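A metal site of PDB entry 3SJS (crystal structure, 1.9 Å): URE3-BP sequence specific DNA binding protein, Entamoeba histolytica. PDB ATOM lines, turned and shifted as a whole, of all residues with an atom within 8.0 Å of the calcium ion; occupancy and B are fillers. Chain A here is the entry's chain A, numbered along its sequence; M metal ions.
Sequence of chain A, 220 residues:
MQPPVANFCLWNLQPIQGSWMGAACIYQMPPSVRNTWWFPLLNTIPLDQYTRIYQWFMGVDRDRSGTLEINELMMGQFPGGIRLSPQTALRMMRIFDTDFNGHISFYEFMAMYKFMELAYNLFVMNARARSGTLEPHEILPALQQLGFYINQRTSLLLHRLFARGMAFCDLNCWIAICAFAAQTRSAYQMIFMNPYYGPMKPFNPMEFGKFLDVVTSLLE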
ATOM      1  N   PHE A  57     -22.787 -35.930  -5.426  1.00  0.00           N
ATOM      2  CA  PHE A  57     -21.697 -34.997  -5.665  1.00  0.00           C
ATOM      3  C   PHE A  57     -21.707 -34.512  -7.103  1.00  0.00           C
ATOM      4  O   PHE A  57     -21.560 -33.343  -7.364  1.00  0.00           O
ATOM      5  CB  PHE A  57     -20.368 -35.701  -5.344  1.00  0.00           C
ATOM      6  CG  PHE A  57     -19.143 -34.834  -5.403  1.00  0.00           C
ATOM      7  CD1 PHE A  57     -18.777 -34.058  -4.319  1.00  0.00           C
ATOM      8  CD2 PHE A  57     -18.333 -34.833  -6.507  1.00  0.00           C
ATOM      9  CE1 PHE A  57     -17.618 -33.305  -4.317  1.00  0.00           C
ATOM     10  CE2 PHE A  57     -17.159 -34.052  -6.503  1.00  0.00           C
ATOM     11  CZ  PHE A  57     -16.831 -33.294  -5.399  1.00  0.00           C
ATOM     12  N   VAL A  60     -24.326 -31.846  -7.770  1.00  0.00           N
ATOM     13  CA  VAL A  60     -24.048 -30.545  -7.142  1.00  0.00           C
ATOM     14  C   VAL A  60     -22.811 -29.864  -7.774  1.00  0.00           C
ATOM     15  O   VAL A  60     -22.673 -28.651  -7.706  1.00  0.00           O
ATOM     16  CB  VAL A  60     -23.819 -30.761  -5.625  1.00  0.00           C
ATOM     17  CG1 VAL A  60     -23.503 -29.487  -4.898  1.00  0.00           C
ATOM     18  CG2 VAL A  60     -25.049 -31.389  -5.019  1.00  0.00           C
ATOM     19  N   ASP A  61     -21.930 -30.653  -8.384  1.00  0.00           N
ATOM     20  CA  ASP A  61     -20.698 -30.160  -9.047  1.00  0.00           C
ATOM     21  C   ASP A  61     -20.968 -29.554 -10.412  1.00  0.00           C
ATOM     22  O   ASP A  61     -20.751 -30.180 -11.462  1.00  0.00           O
ATOM     23  CB  ASP A  61     -19.669 -31.299  -9.181  1.00  0.00           C
ATOM     24  CG  ASP A  61     -18.340 -30.841  -9.801  1.00  0.00           C
ATOM     25  OD1 ASP A  61     -18.132 -29.627  -9.996  1.00  0.00           O
ATOM     26  OD2 ASP A  61     -17.489 -31.713 -10.081  1.00  0.00           O
ATOM     27  N   ARG A  62     -21.396 -28.300 -10.400  1.00  0.00           N
ATOM     28  CA  ARG A  62     -21.855 -27.629 -11.607  1.00  0.00           C
ATOM     29  C   ARG A  62     -20.783 -27.434 -12.700  1.00  0.00           C
ATOM     30  O   ARG A  62     -21.118 -27.386 -13.866  1.00  0.00           O
ATOM     31  CB  ARG A  62     -22.438 -26.264 -11.230  1.00  0.00           C
ATOM     32  CG  ARG A  62     -23.653 -26.298 -10.323  1.00  0.00           C
ATOM     33  CD  ARG A  62     -24.222 -24.893 -10.093  1.00  0.00           C
ATOM     34  NE  ARG A  62     -24.732 -24.330 -11.355  1.00  0.00           N
ATOM     35  CZ  ARG A  62     -25.887 -24.667 -11.923  1.00  0.00           C
ATOM     36  NH1 ARG A  62     -26.689 -25.562 -11.348  1.00  0.00           N
ATOM     37  NH2 ARG A  62     -26.237 -24.117 -13.078  1.00  0.00           N
ATOM     38  N   ASP A  63     -19.503 -27.338 -12.362  1.00  0.00           N
ATOM     39  CA  ASP A  63     -18.489 -27.106 -13.417  1.00  0.00           C
ATOM     40  C   ASP A  63     -17.599 -28.326 -13.693  1.00  0.00           C
ATOM     41  O   ASP A  63     -16.553 -28.193 -14.284  1.00  0.00           O
ATOM     42  CB  ASP A  63     -17.687 -25.852 -13.094  1.00  0.00           C
ATOM     43  CG  ASP A  63     -16.889 -25.935 -11.835  1.00  0.00           C
ATOM     44  OD1 ASP A  63     -16.953 -26.932 -11.096  1.00  0.00           O
ATOM     45  OD2 ASP A  63     -16.149 -24.980 -11.553  1.00  0.00           O
ATOM     46  N   ARG A  64     -18.036 -29.491 -13.235  1.00  0.00           N
ATOM     47  CA  ARG A  64     -17.261 -30.751 -13.313  1.00  0.00           C
ATOM     48  C   ARG A  64     -15.787 -30.656 -12.867  1.00  0.00           C
ATOM     49  O   ARG A  64     -14.931 -31.308 -13.464  1.00  0.00           O
ATOM     50  CB  ARG A  64     -17.337 -31.297 -14.712  1.00  0.00           C
ATOM     51  CG  ARG A  64     -18.709 -31.763 -15.085  1.00  0.00           C
ATOM     52  CD  ARG A  64     -18.680 -32.294 -16.491  1.00  0.00           C
ATOM     53  NE  ARG A  64     -17.858 -33.498 -16.551  1.00  0.00           N
ATOM     54  CZ  ARG A  64     -17.038 -33.842 -17.546  1.00  0.00           C
ATOM     55  NH1 ARG A  64     -16.880 -33.087 -18.629  1.00  0.00           N
ATOM     56  NH2 ARG A  64     -16.366 -34.969 -17.419  1.00  0.00           N
ATOM     57  N   SER A  65     -15.518 -29.880 -11.819  1.00  0.00           N
ATOM     58  CA  SER A  65     -14.176 -29.697 -11.321  1.00  0.00           C
ATOM     59  C   SER A  65     -13.758 -30.842 -10.416  1.00  0.00           C
ATOM     60  O   SER A  65     -12.568 -30.985 -10.106  1.00  0.00           O
ATOM     61  CB  SER A  65     -14.047 -28.370 -10.550  1.00  0.00           C
ATOM     62  OG  SER A  65     -14.904 -28.327  -9.437  1.00  0.00           O
ATOM     63  N   GLY A  66     -14.723 -31.646  -9.976  1.00  0.00           N
ATOM     64  CA  GLY A  66     -14.478 -32.691  -8.985  1.00  0.00           C
ATOM     65  C   GLY A  66     -14.303 -32.132  -7.584  1.00  0.00           C
ATOM     66  O   GLY A  66     -13.803 -32.820  -6.689  1.00  0.00           O
ATOM     67  N   THR A  67     -14.706 -30.877  -7.389  1.00  0.00           N
ATOM     68  CA  THR A  67     -14.656 -30.228  -6.121  1.00  0.00           C
ATOM     69  C   THR A  67     -15.893 -29.323  -6.053  1.00  0.00           C
ATOM     70  O   THR A  67     -16.500 -28.991  -7.068  1.00  0.00           O
ATOM     71  CB  THR A  67     -13.413 -29.382  -5.967  1.00  0.00           C
ATOM     72  OG1 THR A  67     -13.443 -28.355  -6.937  1.00  0.00           O
ATOM     73  CG2 THR A  67     -12.147 -30.222  -6.143  1.00  0.00           C
ATOM     74  N   LEU A  68     -16.276 -28.949  -4.849  1.00  0.00           N
ATOM     75  CA  LEU A  68     -17.410 -28.084  -4.670  1.00  0.00           C
ATOM     76  C   LEU A  68     -16.943 -26.798  -4.041  1.00  0.00           C
ATOM     77  O   LEU A  68     -16.132 -26.781  -3.111  1.00  0.00           O
ATOM     78  CB  LEU A  68     -18.490 -28.728  -3.826  1.00  0.00           C
ATOM     79  CG  LEU A  68     -19.102 -30.053  -4.294  1.00  0.00           C
ATOM     80  CD1 LEU A  68     -20.079 -30.523  -3.258  1.00  0.00           C
ATOM     81  CD2 LEU A  68     -19.743 -29.883  -5.674  1.00  0.00           C
ATOM     82  N   GLU A  69     -17.477 -25.724  -4.577  1.00  0.00           N
ATOM     83  CA  GLU A  69     -17.185 -24.411  -4.139  1.00  0.00           C
ATOM     84  C   GLU A  69     -18.448 -23.954  -3.399  1.00  0.00           C
ATOM     85  O   GLU A  69     -19.503 -24.599  -3.445  1.00  0.00           O
ATOM     86  CB  GLU A  69     -16.859 -23.531  -5.366  1.00  0.00           C
ATOM     87  CG  GLU A  69     -15.546 -23.919  -6.122  1.00  0.00           C
ATOM     88  CD  GLU A  69     -15.436 -25.403  -6.648  1.00  0.00           C
ATOM     89  OE1 GLU A  69     -16.227 -25.817  -7.545  1.00  0.00           O
ATOM     90  OE2 GLU A  69     -14.469 -26.133  -6.226  1.00  0.00           O
ATOM     91  N   ILE A  70     -18.337 -22.865  -2.663  1.00  0.00           N
ATOM     92  CA  ILE A  70     -19.451 -22.440  -1.815  1.00  0.00           C
ATOM     93  C   ILE A  70     -20.727 -22.143  -2.660  1.00  0.00           C
ATOM     94  O   ILE A  70     -21.852 -22.384  -2.220  1.00  0.00           O
ATOM     95  CB  ILE A  70     -19.039 -21.230  -0.910  1.00  0.00           C
ATOM     96  CG1 ILE A  70     -20.201 -20.854   0.046  1.00  0.00           C
ATOM     97  CG2 ILE A  70     -18.545 -20.030  -1.800  1.00  0.00           C
ATOM     98  CD1 ILE A  70     -19.828 -19.876   1.152  1.00  0.00           C
ATOM     99  N   GLU A  72     -21.775 -23.716  -5.246  1.00  0.00           N
ATOM    100  CA  GLU A  72     -22.439 -25.016  -5.534  1.00  0.00           C
ATOM    101  C   GLU A  72     -23.150 -25.561  -4.284  1.00  0.00           C
ATOM    102  O   GLU A  72     -24.191 -26.193  -4.380  1.00  0.00           O
ATOM    103  CB  GLU A  72     -21.401 -26.026  -6.071  1.00  0.00           C
ATOM    104  CG  GLU A  72     -20.949 -25.684  -7.484  1.00  0.00           C
ATOM    105  CD  GLU A  72     -19.561 -26.175  -7.883  1.00  0.00           C
ATOM    106  OE1 GLU A  72     -18.655 -26.197  -7.050  1.00  0.00           O
ATOM    107  OE2 GLU A  72     -19.360 -26.490  -9.064  1.00  0.00           O
ATOM    108  N   HIS A 103     -12.369 -24.903  -1.671  1.00  0.00           N
ATOM    109  CA  HIS A 103     -13.054 -26.027  -2.316  1.00  0.00           C
ATOM    110  C   HIS A 103     -13.190 -27.172  -1.337  1.00  0.00           C
ATOM    111  O   HIS A 103     -12.329 -27.374  -0.489  1.00  0.00           O
ATOM    112  CB  HIS A 103     -12.241 -26.611  -3.465  1.00  0.00           C
ATOM    113  CG  HIS A 103     -11.651 -25.590  -4.371  1.00  0.00           C
ATOM    114  ND1 HIS A 103     -12.434 -24.666  -5.042  1.00  0.00           N
ATOM    115  CD2 HIS A 103     -10.371 -25.344  -4.719  1.00  0.00           C
ATOM    116  CE1 HIS A 103     -11.655 -23.880  -5.752  1.00  0.00           C
ATOM    117  NE2 HIS A 103     -10.394 -24.263  -5.574  1.00  0.00           N
ATOM    118  N   ILE A 104     -14.262 -27.950  -1.491  1.00  0.00           N
ATOM    119  CA  ILE A 104     -14.459 -29.192  -0.762  1.00  0.00           C
ATOM    120  C   ILE A 104     -14.194 -30.351  -1.740  1.00  0.00           C
ATOM    121  O   ILE A 104     -14.764 -30.390  -2.807  1.00  0.00           O
ATOM    122  CB  ILE A 104     -15.884 -29.208  -0.200  1.00  0.00           C
ATOM    123  CG1 ILE A 104     -15.911 -28.401   1.096  1.00  0.00           C
ATOM    124  CG2 ILE A 104     -16.362 -30.599   0.068  1.00  0.00           C
ATOM    125  CD1 ILE A 104     -17.317 -28.210   1.627  1.00  0.00           C
HETATM  126 CA    CA M   1     -17.143 -27.702  -8.867  1.00  0.00          CA
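The calcium ion is bound by O of Thr 67.
The calcium ion is bound by OD1 of Asp 63 (2.4 Å).
The side-chain hydroxyl (OG) of Ser 65 binds the calcium ion.
The calcium ion is bound by OD1 of Asp 61 (2.4 Å).
OE1 of Glu 69 binds the calcium ion (2.5 Å).
The side-chain carboxylate (OE2) of Glu 72 binds the calcium ion.
The calcium ion is bound by the side-chain carboxylate (OE1) of Glu 72.
The calcium ion has seven donor atoms within binding distance.
OD2 of Asp 61 sits at hydrogen-bond distance from N of Gly 66 (2.8 Å).
The backbone NH of Arg 64 sits close to the side-chain carboxylate of Asp 61, 3.2 Å away.
The side-chain carboxylate of Glu 69 lies within hydrogen-bond range of a ring nitrogen (ND1) of His 103 (2.8 Å).
The backbone NH (N) of Arg 62 sits close to the side-chain carboxylate (OE2) of Glu 72 (3.0 Å).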
